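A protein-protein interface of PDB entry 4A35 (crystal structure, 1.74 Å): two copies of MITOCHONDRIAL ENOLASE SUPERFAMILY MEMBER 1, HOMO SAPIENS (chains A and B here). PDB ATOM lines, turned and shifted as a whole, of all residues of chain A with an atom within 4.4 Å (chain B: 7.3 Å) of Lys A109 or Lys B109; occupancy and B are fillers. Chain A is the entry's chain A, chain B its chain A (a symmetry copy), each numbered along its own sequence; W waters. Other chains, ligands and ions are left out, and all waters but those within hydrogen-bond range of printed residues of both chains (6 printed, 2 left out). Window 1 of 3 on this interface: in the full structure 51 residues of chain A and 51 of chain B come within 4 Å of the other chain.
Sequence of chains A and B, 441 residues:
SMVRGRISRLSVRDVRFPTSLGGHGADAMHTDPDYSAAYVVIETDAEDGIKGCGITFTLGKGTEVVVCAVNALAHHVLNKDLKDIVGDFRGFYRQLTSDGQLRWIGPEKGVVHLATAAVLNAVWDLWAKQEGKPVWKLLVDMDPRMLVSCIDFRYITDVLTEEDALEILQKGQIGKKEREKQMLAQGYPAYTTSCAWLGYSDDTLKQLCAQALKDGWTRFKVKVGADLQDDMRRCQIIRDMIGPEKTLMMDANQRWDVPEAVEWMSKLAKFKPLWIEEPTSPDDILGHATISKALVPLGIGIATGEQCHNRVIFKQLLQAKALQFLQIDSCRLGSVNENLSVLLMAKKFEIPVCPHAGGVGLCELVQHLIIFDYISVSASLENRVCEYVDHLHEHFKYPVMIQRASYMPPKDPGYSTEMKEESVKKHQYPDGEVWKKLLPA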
ATOM      1  N   GLY A 106     -26.885  27.392  27.229  1.00  0.00           N
ATOM      2  CA  GLY A 106     -25.631  26.645  27.248  1.00  0.00           C
ATOM      3  C   GLY A 106     -24.982  26.983  25.905  1.00  0.00           C
ATOM      4  O   GLY A 106     -24.521  28.111  25.715  1.00  0.00           O
ATOM      5  N   PRO A 107     -25.069  26.087  24.886  1.00  0.00           N
ATOM      6  CA  PRO A 107     -25.571  24.710  24.973  1.00  0.00           C
ATOM      7  C   PRO A 107     -24.544  23.757  25.584  1.00  0.00           C
ATOM      8  O   PRO A 107     -23.329  23.848  25.305  1.00  0.00           O
ATOM      9  CB  PRO A 107     -25.818  24.310  23.496  1.00  0.00           C
ATOM     10  CG  PRO A 107     -25.167  25.359  22.658  1.00  0.00           C
ATOM     11  CD  PRO A 107     -24.524  26.381  23.543  1.00  0.00           C
ATOM     12  N   GLU A 108     -25.043  22.809  26.421  1.00  0.00           N
ATOM     13  CA  GLU A 108     -24.218  21.777  27.056  1.00  0.00           C
ATOM     14  C   GLU A 108     -22.963  22.365  27.748  1.00  0.00           C
ATOM     15  O   GLU A 108     -21.842  21.862  27.611  1.00  0.00           O
ATOM     16  CB  GLU A 108     -23.839  20.664  26.062  1.00  0.00           C
ATOM     17  CG  GLU A 108     -25.003  19.728  25.774  1.00  0.00           C
ATOM     18  CD  GLU A 108     -24.540  18.385  25.243  1.00  0.00           C
ATOM     19  OE1 GLU A 108     -24.032  18.347  24.101  1.00  0.00           O
ATOM     20  OE2 GLU A 108     -24.593  17.390  25.996  1.00  0.00           O
ATOM     21  N   LYS A 109     -23.181  23.441  28.546  1.00  0.00           N
ATOM     22  CA  LYS A 109     -22.094  24.057  29.324  1.00  0.00           C
ATOM     23  C   LYS A 109     -22.669  24.910  30.436  1.00  0.00           C
ATOM     24  O   LYS A 109     -23.787  25.398  30.341  1.00  0.00           O
ATOM     25  CB  LYS A 109     -21.170  24.911  28.427  1.00  0.00           C
ATOM     26  CG  LYS A 109     -21.866  26.159  27.852  1.00  0.00           C
ATOM     27  CD  LYS A 109     -20.990  26.855  26.750  1.00  0.00           C
ATOM     28  CE  LYS A 109     -20.866  26.035  25.485  1.00  0.00           C
ATOM     29  NZ  LYS A 109     -20.417  26.919  24.378  1.00  0.00           N
ATOM     30  N   GLY A 110     -21.869  25.162  31.454  1.00  0.00           N
ATOM     31  CA  GLY A 110     -22.320  25.995  32.543  1.00  0.00           C
ATOM     32  C   GLY A 110     -23.495  25.421  33.323  1.00  0.00           C
ATOM     33  O   GLY A 110     -23.698  24.179  33.416  1.00  0.00           O
ATOM     34  N   VAL A 111     -24.295  26.356  33.848  1.00  0.00           N
ATOM     35  CA  VAL A 111     -25.432  26.062  34.744  1.00  0.00           C
ATOM     36  C   VAL A 111     -26.363  24.998  34.177  1.00  0.00           C
ATOM     37  O   VAL A 111     -26.713  24.028  34.884  1.00  0.00           O
ATOM     38  CB  VAL A 111     -26.214  27.342  35.092  1.00  0.00           C
ATOM     39  CG1 VAL A 111     -27.595  26.997  35.683  1.00  0.00           C
ATOM     40  CG2 VAL A 111     -25.395  28.189  36.073  1.00  0.00           C
ATOM     41  N   VAL A 112     -26.740  25.156  32.919  1.00  0.00           N
ATOM     42  CA  VAL A 112     -27.762  24.260  32.338  1.00  0.00           C
ATOM     43  C   VAL A 112     -27.229  22.797  32.288  1.00  0.00           C
ATOM     44  O   VAL A 112     -28.008  21.876  32.554  1.00  0.00           O
ATOM     45  CB  VAL A 112     -28.282  24.756  30.949  1.00  0.00           C
ATOM     46  CG1 VAL A 112     -27.224  24.589  29.852  1.00  0.00           C
ATOM     47  CG2 VAL A 112     -29.612  24.067  30.574  1.00  0.00           C
ATOM     48  N   HIS A 113     -25.923  22.620  32.056  1.00  0.00           N
ATOM     49  CA  HIS A 113     -25.342  21.261  32.002  1.00  0.00           C
ATOM     50  C   HIS A 113     -25.155  20.679  33.405  1.00  0.00           C
ATOM     51  O   HIS A 113     -25.372  19.466  33.613  1.00  0.00           O
ATOM     52  CB  HIS A 113     -24.051  21.236  31.198  1.00  0.00           C
ATOM     53  CG  HIS A 113     -23.890  19.977  30.390  1.00  0.00           C
ATOM     54  ND1 HIS A 113     -24.900  19.514  29.562  1.00  0.00           N
ATOM     55  CD2 HIS A 113     -22.782  19.215  30.200  1.00  0.00           C
ATOM     56  CE1 HIS A 113     -24.425  18.407  29.013  1.00  0.00           C
ATOM     57  NE2 HIS A 113     -23.129  18.230  29.318  1.00  0.00           N
ATOM     58  N   ASP A 283     -10.913  25.705  28.744  1.00  0.00           N
ATOM     59  CA  ASP A 283     -11.332  25.789  27.315  1.00  0.00           C
ATOM     60  C   ASP A 283     -10.154  25.783  26.338  1.00  0.00           C
ATOM     61  O   ASP A 283     -10.363  25.702  25.116  1.00  0.00           O
ATOM     62  CB  ASP A 283     -12.087  27.116  27.061  1.00  0.00           C
ATOM     63  CG  ASP A 283     -13.371  27.272  27.837  1.00  0.00           C
ATOM     64  OD1 ASP A 283     -14.176  26.312  27.857  1.00  0.00           O
ATOM     65  OD2 ASP A 283     -13.604  28.373  28.372  1.00  0.00           O
ATOM     66  N   GLN A 307     -13.129  20.762  34.803  1.00  0.00           N
ATOM     67  CA  GLN A 307     -14.081  21.807  34.459  1.00  0.00           C
ATOM     68  C   GLN A 307     -14.349  21.805  32.953  1.00  0.00           C
ATOM     69  O   GLN A 307     -14.979  22.738  32.440  1.00  0.00           O
ATOM     70  CB  GLN A 307     -13.584  23.203  34.932  1.00  0.00           C
ATOM     71  CG  GLN A 307     -13.667  23.339  36.471  1.00  0.00           C
ATOM     72  CD  GLN A 307     -14.034  24.738  36.938  1.00  0.00           C
ATOM     73  OE1 GLN A 307     -13.246  25.427  37.609  1.00  0.00           O
ATOM     74  NE2 GLN A 307     -15.281  25.141  36.732  1.00  0.00           N
ATOM     75  N   HIS A 309     -16.232  21.330  29.978  1.00  0.00           N
ATOM     76  CA  HIS A 309     -17.706  21.345  29.966  1.00  0.00           C
ATOM     77  C   HIS A 309     -18.486  20.254  29.210  1.00  0.00           C
ATOM     78  O   HIS A 309     -19.642  19.986  29.590  1.00  0.00           O
ATOM     79  CB  HIS A 309     -18.258  22.761  29.651  1.00  0.00           C
ATOM     80  CG  HIS A 309     -17.840  23.330  28.329  1.00  0.00           C
ATOM     81  ND1 HIS A 309     -18.522  23.012  27.174  1.00  0.00           N
ATOM     82  CD2 HIS A 309     -16.811  24.150  28.020  1.00  0.00           C
ATOM     83  CE1 HIS A 309     -17.920  23.670  26.198  1.00  0.00           C
ATOM     84  NE2 HIS A 309     -16.868  24.338  26.641  1.00  0.00           N
ATOM     85  N   THR B  97     -16.418  37.844  36.541  1.00  0.00           N
ATOM     86  CA  THR B  97     -16.173  36.620  35.738  1.00  0.00           C
ATOM     87  C   THR B  97     -15.275  35.575  36.447  1.00  0.00           C
ATOM     88  O   THR B  97     -15.203  34.426  35.977  1.00  0.00           O
ATOM     89  CB  THR B  97     -15.528  37.017  34.376  1.00  0.00           C
ATOM     90  OG1 THR B  97     -14.295  37.665  34.663  1.00  0.00           O
ATOM     91  CG2 THR B  97     -16.436  37.856  33.485  1.00  0.00           C
ATOM     92  N   ARG B 103     -17.538  31.503  39.780  1.00  0.00           N
ATOM     93  CA  ARG B 103     -16.886  31.098  38.520  1.00  0.00           C
ATOM     94  C   ARG B 103     -17.036  29.550  38.288  1.00  0.00           C
ATOM     95  O   ARG B 103     -17.015  29.091  37.144  1.00  0.00           O
ATOM     96  CB  ARG B 103     -15.380  31.503  38.517  1.00  0.00           C
ATOM     97  CG  ARG B 103     -14.514  30.624  39.450  1.00  0.00           C
ATOM     98  CD  ARG B 103     -13.051  31.114  39.542  1.00  0.00           C
ATOM     99  NE  ARG B 103     -12.485  31.428  38.221  1.00  0.00           N
ATOM    100  CZ  ARG B 103     -12.035  30.519  37.356  1.00  0.00           C
ATOM    101  NH1 ARG B 103     -12.090  29.218  37.655  1.00  0.00           N
ATOM    102  NH2 ARG B 103     -11.522  30.898  36.195  1.00  0.00           N
ATOM    103  N   ILE B 105     -19.658  27.851  38.370  1.00  0.00           N
ATOM    104  CA  ILE B 105     -20.848  27.548  37.577  1.00  0.00           C
ATOM    105  C   ILE B 105     -20.689  27.958  36.078  1.00  0.00           C
ATOM    106  O   ILE B 105     -21.606  27.707  35.288  1.00  0.00           O
ATOM    107  CB  ILE B 105     -22.151  28.011  38.191  1.00  0.00           C
ATOM    108  CG1 ILE B 105     -22.259  29.553  38.188  1.00  0.00           C
ATOM    109  CG2 ILE B 105     -22.362  27.353  39.617  1.00  0.00           C
ATOM    110  CD1 ILE B 105     -23.748  30.065  38.625  1.00  0.00           C
ATOM    111  N   GLY B 106     -19.515  28.468  35.717  1.00  0.00           N
ATOM    112  CA  GLY B 106     -19.121  28.708  34.332  1.00  0.00           C
ATOM    113  C   GLY B 106     -17.909  27.795  34.133  1.00  0.00           C
ATOM    114  O   GLY B 106     -18.067  26.574  34.071  1.00  0.00           O
ATOM    115  N   PRO B 107     -16.662  28.334  34.190  1.00  0.00           N
ATOM    116  CA  PRO B 107     -16.328  29.762  34.242  1.00  0.00           C
ATOM    117  C   PRO B 107     -16.442  30.434  32.873  1.00  0.00           C
ATOM    118  O   PRO B 107     -16.065  29.852  31.833  1.00  0.00           O
ATOM    119  CB  PRO B 107     -14.846  29.781  34.695  1.00  0.00           C
ATOM    120  CG  PRO B 107     -14.350  28.379  34.582  1.00  0.00           C
ATOM    121  CD  PRO B 107     -15.449  27.497  34.075  1.00  0.00           C
ATOM    122  N   GLU B 108     -16.953  31.693  32.873  1.00  0.00           N
ATOM    123  CA  GLU B 108     -17.085  32.512  31.666  1.00  0.00           C
ATOM    124  C   GLU B 108     -17.780  31.751  30.508  1.00  0.00           C
ATOM    125  O   GLU B 108     -17.342  31.773  29.353  1.00  0.00           O
ATOM    126  CB  GLU B 108     -15.729  33.089  31.221  1.00  0.00           C
ATOM    127  CG  GLU B 108     -15.280  34.246  32.101  1.00  0.00           C
ATOM    128  CD  GLU B 108     -14.264  35.133  31.405  1.00  0.00           C
ATOM    129  OE1 GLU B 108     -13.127  34.664  31.184  1.00  0.00           O
ATOM    130  OE2 GLU B 108     -14.627  36.256  30.997  1.00  0.00           O
ATOM    131  N   LYS B 109     -18.921  31.095  30.837  1.00  0.00           N
ATOM    132  CA  LYS B 109     -19.725  30.391  29.824  1.00  0.00           C
ATOM    133  C   LYS B 109     -21.125  30.147  30.350  1.00  0.00           C
ATOM    134  O   LYS B 109     -21.341  30.071  31.552  1.00  0.00           O
ATOM    135  CB  LYS B 109     -19.073  29.051  29.415  1.00  0.00           C
ATOM    136  CG  LYS B 109     -19.055  28.012  30.553  1.00  0.00           C
ATOM    137  CD  LYS B 109     -18.164  26.771  30.189  1.00  0.00           C
ATOM    138  CE  LYS B 109     -16.688  27.098  30.128  1.00  0.00           C
ATOM    139  NZ  LYS B 109     -15.910  25.835  30.218  1.00  0.00           N
ATOM    140  N   GLY B 110     -22.061  29.938  29.445  1.00  0.00           N
ATOM    141  CA  GLY B 110     -23.417  29.662  29.855  1.00  0.00           C
ATOM    142  C   GLY B 110     -24.088  30.805  30.605  1.00  0.00           C
ATOM    143  O   GLY B 110     -23.770  32.012  30.416  1.00  0.00           O
ATOM    144  N   VAL B 111     -24.998  30.397  31.497  1.00  0.00           N
ATOM    145  CA  VAL B 111     -25.868  31.310  32.265  1.00  0.00           C
ATOM    146  C   VAL B 111     -25.085  32.420  32.956  1.00  0.00           C
ATOM    147  O   VAL B 111     -25.450  33.611  32.841  1.00  0.00           O
ATOM    148  CB  VAL B 111     -26.731  30.538  33.281  1.00  0.00           C
ATOM    149  CG1 VAL B 111     -27.329  31.493  34.332  1.00  0.00           C
ATOM    150  CG2 VAL B 111     -27.837  29.779  32.538  1.00  0.00           C
ATOM    151  N   VAL B 112     -24.016  32.049  33.640  1.00  0.00           N
ATOM    152  CA  VAL B 112     -23.290  33.035  34.466  1.00  0.00           C
ATOM    153  C   VAL B 112     -22.673  34.145  33.562  1.00  0.00           C
ATOM    154  O   VAL B 112     -22.696  35.313  33.962  1.00  0.00           O
ATOM    155  CB  VAL B 112     -22.233  32.374  35.410  1.00  0.00           C
ATOM    156  CG1 VAL B 112     -21.027  31.842  34.629  1.00  0.00           C
ATOM    157  CG2 VAL B 112     -21.809  33.342  36.535  1.00  0.00           C
ATOM    158  N   HIS B 113     -22.237  33.784  32.350  1.00  0.00           N
ATOM    159  CA  HIS B 113     -21.645  34.781  31.432  1.00  0.00           C
ATOM    160  C   HIS B 113     -22.725  35.639  30.769  1.00  0.00           C
ATOM    161  O   HIS B 113     -22.526  36.856  30.576  1.00  0.00           O
ATOM    162  CB  HIS B 113     -20.731  34.126  30.407  1.00  0.00           C
ATOM    163  CG  HIS B 113     -19.524  34.963  30.081  1.00  0.00           C
ATOM    164  ND1 HIS B 113     -18.717  35.489  31.077  1.00  0.00           N
ATOM    165  CD2 HIS B 113     -18.948  35.205  28.875  1.00  0.00           C
ATOM    166  CE1 HIS B 113     -17.765  36.156  30.443  1.00  0.00           C
ATOM    167  NE2 HIS B 113     -17.829  35.952  29.117  1.00  0.00           N
ATOM    168  N   LEU B 114     -23.876  35.029  30.410  1.00  0.00           N
ATOM    169  CA  LEU B 114     -25.022  35.801  29.892  1.00  0.00           C
ATOM    170  C   LEU B 114     -25.457  36.855  30.927  1.00  0.00           C
ATOM    171  O   LEU B 114     -25.609  38.048  30.584  1.00  0.00           O
ATOM    172  CB  LEU B 114     -26.193  34.848  29.597  1.00  0.00           C
ATOM    173  CG  LEU B 114     -25.936  33.828  28.446  1.00  0.00           C
ATOM    174  CD1 LEU B 114     -27.179  33.027  28.195  1.00  0.00           C
ATOM    175  CD2 LEU B 114     -25.586  34.562  27.112  1.00  0.00           C
ATOM    176  N   SER B 281     -20.908  22.213  16.043  1.00  0.00           N
ATOM    177  CA  SER B 281     -20.862  22.644  17.462  1.00  0.00           C
ATOM    178  C   SER B 281     -20.037  23.969  17.606  1.00  0.00           C
ATOM    179  O   SER B 281     -18.913  24.034  17.084  1.00  0.00           O
ATOM    180  CB  SER B 281     -20.260  21.548  18.328  1.00  0.00           C
ATOM    181  OG  SER B 281     -19.882  22.075  19.590  1.00  0.00           O
ATOM    182  N   PRO B 282     -20.551  24.961  18.379  1.00  0.00           N
ATOM    183  CA  PRO B 282     -19.833  26.246  18.557  1.00  0.00           C
ATOM    184  C   PRO B 282     -18.551  26.056  19.372  1.00  0.00           C
ATOM    185  O   PRO B 282     -17.735  26.963  19.410  1.00  0.00           O
ATOM    186  CB  PRO B 282     -20.855  27.102  19.311  1.00  0.00           C
ATOM    187  CG  PRO B 282     -21.578  26.077  20.184  1.00  0.00           C
ATOM    188  CD  PRO B 282     -21.805  24.966  19.168  1.00  0.00           C
ATOM    189  N   ASP B 283     -18.392  24.882  20.029  1.00  0.00           N
ATOM    190  CA  ASP B 283     -17.143  24.543  20.770  1.00  0.00           C
ATOM    191  C   ASP B 283     -16.088  23.860  19.896  1.00  0.00           C
ATOM    192  O   ASP B 283     -14.949  23.655  20.347  1.00  0.00           O
ATOM    193  CB  ASP B 283     -17.458  23.546  21.911  1.00  0.00           C
ATOM    194  CG  ASP B 283     -18.390  24.073  22.973  1.00  0.00           C
ATOM    195  OD1 ASP B 283     -18.175  25.215  23.442  1.00  0.00           O
ATOM    196  OD2 ASP B 283     -19.298  23.324  23.382  1.00  0.00           O
ATOM    197  N   GLN B 307     -22.588  31.803  19.287  1.00  0.00           N
ATOM    198  CA  GLN B 307     -22.746  31.101  20.550  1.00  0.00           C
ATOM    199  C   GLN B 307     -21.377  30.763  21.144  1.00  0.00           C
ATOM    200  O   GLN B 307     -21.299  30.001  22.115  1.00  0.00           O
ATOM    201  CB  GLN B 307     -23.609  29.817  20.380  1.00  0.00           C
ATOM    202  CG  GLN B 307     -25.098  30.167  20.145  1.00  0.00           C
ATOM    203  CD  GLN B 307     -26.060  29.178  20.781  1.00  0.00           C
ATOM    204  OE1 GLN B 307     -26.827  28.482  20.092  1.00  0.00           O
ATOM    205  NE2 GLN B 307     -26.160  29.190  22.104  1.00  0.00           N
ATOM    206  N   CYS B 308     -20.282  31.301  20.520  1.00  0.00           N
ATOM    207  CA  CYS B 308     -18.933  31.127  21.007  1.00  0.00           C
ATOM    208  C   CYS B 308     -18.842  31.768  22.403  1.00  0.00           C
ATOM    209  O   CYS B 308     -19.051  32.984  22.512  1.00  0.00           O
ATOM    210  CB  CYS B 308     -17.970  31.777  20.040  1.00  0.00           C
ATOM    211  SG  CYS B 308     -16.293  31.705  20.618  1.00  0.00           S
ATOM    212  N   HIS B 309     -18.674  30.986  23.440  1.00  0.00           N
ATOM    213  CA  HIS B 309     -18.849  31.479  24.818  1.00  0.00           C
ATOM    214  C   HIS B 309     -17.862  32.506  25.403  1.00  0.00           C
ATOM    215  O   HIS B 309     -18.264  33.254  26.315  1.00  0.00           O
ATOM    216  CB  HIS B 309     -19.113  30.315  25.810  1.00  0.00           C
ATOM    217  CG  HIS B 309     -18.029  29.283  25.886  1.00  0.00           C
ATOM    218  ND1 HIS B 309     -16.927  29.471  26.694  1.00  0.00           N
ATOM    219  CD2 HIS B 309     -17.900  28.105  25.235  1.00  0.00           C
ATOM    220  CE1 HIS B 309     -16.174  28.396  26.546  1.00  0.00           C
ATOM    221  NE2 HIS B 309     -16.689  27.561  25.658  1.00  0.00           N
ATOM    222  N   ASN B 310     -16.597  32.556  24.949  1.00  0.00           N
ATOM    223  CA  ASN B 310     -15.680  33.554  25.515  1.00  0.00           C
ATOM    224  C   ASN B 310     -14.520  33.746  24.546  1.00  0.00           C
ATOM    225  O   ASN B 310     -14.458  33.080  23.494  1.00  0.00           O
ATOM    226  CB  ASN B 310     -15.234  33.207  26.964  1.00  0.00           C
ATOM    227  CG  ASN B 310     -14.414  31.937  27.113  1.00  0.00           C
ATOM    228  OD1 ASN B 310     -13.673  31.548  26.196  1.00  0.00           O
ATOM    229  ND2 ASN B 310     -14.603  31.232  28.233  1.00  0.00           N
ATOM    230  N   ILE B 313     -12.179  30.703  23.216  1.00  0.00           N
ATOM    231  CA  ILE B 313     -12.663  29.965  22.052  1.00  0.00           C
ATOM    232  C   ILE B 313     -12.306  30.780  20.815  1.00  0.00           C
ATOM    233  O   ILE B 313     -11.801  30.196  19.872  1.00  0.00           O
ATOM    234  CB  ILE B 313     -14.199  29.647  22.131  1.00  0.00           C
ATOM    235  CG1 ILE B 313     -14.559  28.810  23.453  1.00  0.00           C
ATOM    236  CG2 ILE B 313     -14.632  28.847  20.853  1.00  0.00           C
ATOM    237  CD1 ILE B 313     -13.869  27.342  23.466  1.00  0.00           C
ATOM    238  N   ARG B 332     -23.552  37.460  24.296  1.00  0.00           N
ATOM    239  CA  ARG B 332     -23.007  36.133  24.561  1.00  0.00           C
ATOM    240  C   ARG B 332     -21.633  36.286  25.261  1.00  0.00           C
ATOM    241  O   ARG B 332     -21.337  35.594  26.218  1.00  0.00           O
ATOM    242  CB  ARG B 332     -22.819  35.363  23.235  1.00  0.00           C
ATOM    243  CG  ARG B 332     -22.186  33.920  23.444  1.00  0.00           C
ATOM    244  CD  ARG B 332     -23.022  32.990  24.328  1.00  0.00           C
ATOM    245  NE  ARG B 332     -24.378  32.833  23.778  1.00  0.00           N
ATOM    246  CZ  ARG B 332     -25.268  31.945  24.212  1.00  0.00           C
ATOM    247  NH1 ARG B 332     -24.960  31.118  25.215  1.00  0.00           N
ATOM    248  NH2 ARG B 332     -26.467  31.857  23.627  1.00  0.00           N
HETATM  249  O   HOH W   1     -16.899  24.547  32.606  1.00  0.00           O
HETATM  250  O   HOH W   2     -14.014  23.476  28.831  1.00  0.00           O
HETATM  251  O   HOH W   3     -13.988  28.551  30.896  1.00  0.00           O
HETATM  252  O   HOH W   4     -22.313  29.097  24.382  1.00  0.00           O
HETATM  253  O   HOH W   5     -21.754  24.023  23.214  1.00  0.00           O
HETATM  254  O   HOH W   6     -18.080  27.972  22.254  1.00  0.00           O
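The backbone carbonyl oxygen (O) of Gly A106 is in hydrogen-bond range of the guanidinium group (NH1) of Arg B332, at 3.1 Å. The side-chain amino group (NZ) of Lys A109 lies within salt-bridge range of the side-chain carboxylate (OD1) of Asp B283 (3.0 Å). The backbone carbonyl oxygen (O) of Ile B105 lies within hydrogen-bond range of the backbone NH (N) of Val A111 (3.3 Å). The side-chain carboxylate (OD1) of Asp A283 lies within salt-bridge range of the side-chain amino group (NZ) of Lys B109, 3.0 Å away. OD2 of Asp A283 is in hydrogen-bond range of ND2 of Asn B310 (3.0 Å). A ring nitrogen (NE2) of His A309 is in hydrogen-bond range of a ring nitrogen (NE2) of His B309 (3.4 Å).
O of Glu B108 lies within hydrogen-bond range of ND2 of Asn B310, 3.0 Å away. The side-chain hydroxyl (OG) of Ser B281 sits close to the backbone NH (N) of Asp B283, 3.2 Å away. The side-chain amide nitrogen of Gln B307 lies close to the guanidinium group of Arg B332 (3.1 Å). The side-chain sulfur (SG) of Cys B308 lies within hydrogen-bond range of the backbone carbonyl oxygen (O) of Asn B310 (3.7 Å). ND2 of Asn B310 sits at hydrogen-bond distance from ND1 of His B309, at 3.3 Å. The backbone NH of Ile B313 sits at hydrogen-bond distance from the side-chain amide oxygen of Asn B310 (3.4 Å).
Among the printed residues, pairs that only touch across the chains: Lys A109 with His B309 (2.9 Å), His A309 with Lys B109 (2.9 Å), Asp A283 with His B309 (3.2 Å), His A309 with Asp B283 (3.2 Å), Gly A110 with Ile B105 (3.3 Å), Pro A107 with Gln B307 (3.6 Å), Gln A307 with Pro B107 (3.6 Å), Val A111 with Val B111 (3.7 Å), Gln A307 with Lys B109 (3.9 Å), Lys A109 with Gln B307 (3.9 Å), Lys A109 with Lys B109 (3.9 Å) and Gln A307 with Arg B103 (3.96 Å).
Of the printed residues of chain B, Lys A109 touches Lys B109, Asp B283, Gln B307 and His B309. Of chain A, only Lys A109 (3.9 Å), Asp A283 (3.0 Å), Gln A307 (3.9 Å) and His A309 (2.9 Å) come within 4 Å of Lys B109. Of the printed residues of chain B, Gly A110 touches Ile B105 (3.3 Å). Printed residues of chain A within 4 Å of Asn B310: Asp A283. Printed residues of chain A within 4 Å of Asp B283: Lys A109 and His A309. Of the printed residues of chain A, Gln B307 touches Pro A107 and Lys A109. Of the printed residues of chain B, Val A111 touches Ile B105 (3.3 Å) and Val B111 (3.7 Å). Of the printed residues of chain A, Arg B332 touches Gly A106. The nearest residue of chain A that does not touch Lys B109 is Gly A110 (4.1 Å). The nearest printed residue of chain A that does not touch Arg B332 is Pro A107 (5.0 Å).
Hydrophobic or aromatic side chains of chain B that line the printed part of chain A: Ile B105, Pro B107, Val B111 and His B309. Of the 11 printed residues of chain A, 8 touch a printed residue of chain B. Hydrophobic or aromatic side chains of chain A that line the printed part of chain B: Pro A107, Val A111 and His A309. Among the printed residues, Asp or Glu carboxylates within 4 Å of a Lys or Arg side-chain nitrogen of the other chain: Lys A109 with Asp B283 (3.0 Å) and Asp A283 with Lys B109 (3.0 Å).
Pro A107 touches Gln B307, and with the chains exchanged Gln A307 touches Pro B107. Lys A109 touches Asp B283, and with the chains exchanged Asp A283 touches Lys B109. Asp A283 touches His B309, and with the chains exchanged His A309 touches Asp B283. His B309 touches its own counterpart, His A309. Positions printed for both chains: 106, 107, 108, 109, 110, 111, 112, 113, 283, 307 and 309. Of the 18 pairs that touch across the chains among the printed residues, 13 have their exchanged pair printed and touching as well.
Water W3 lies within hydrogen-bond range of OD2 of Asp A283 (2.6 Å), O of Pro B107 (2.6 Å) and NZ of Lys B109 (3.4 Å). Water W5 lies within hydrogen-bond range of the side-chain carboxylate (OD2) of Asp B283 (2.6 Å), the backbone carbonyl oxygen (O) of Pro A107 (2.6 Å) and the side-chain amino group (NZ) of Lys A109 (3.4 Å). Water W4 lies within hydrogen-bond range of O of Gln B307, O of Gly A106, NZ of Lys A109 and NH1 of Arg B332. Water W1 lies within hydrogen-bond range of the backbone carbonyl oxygen of Gln A307, the backbone carbonyl oxygen of Gly B106 and the side-chain amino group of Lys B109. Water W2 lies within hydrogen-bond range of OD1 of Asp A283 (3.0 Å), N of His A309 (3.3 Å) and NZ of Lys B109 (3.3 Å). Water W6 lies within hydrogen-bond range of the side-chain carboxylate of Asp B283 (3.0 Å), the backbone carbonyl oxygen of Pro B282 (3.0 Å), the backbone NH of His B309 (3.3 Å) and the side-chain amino group of Lys A109 (3.3 Å).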
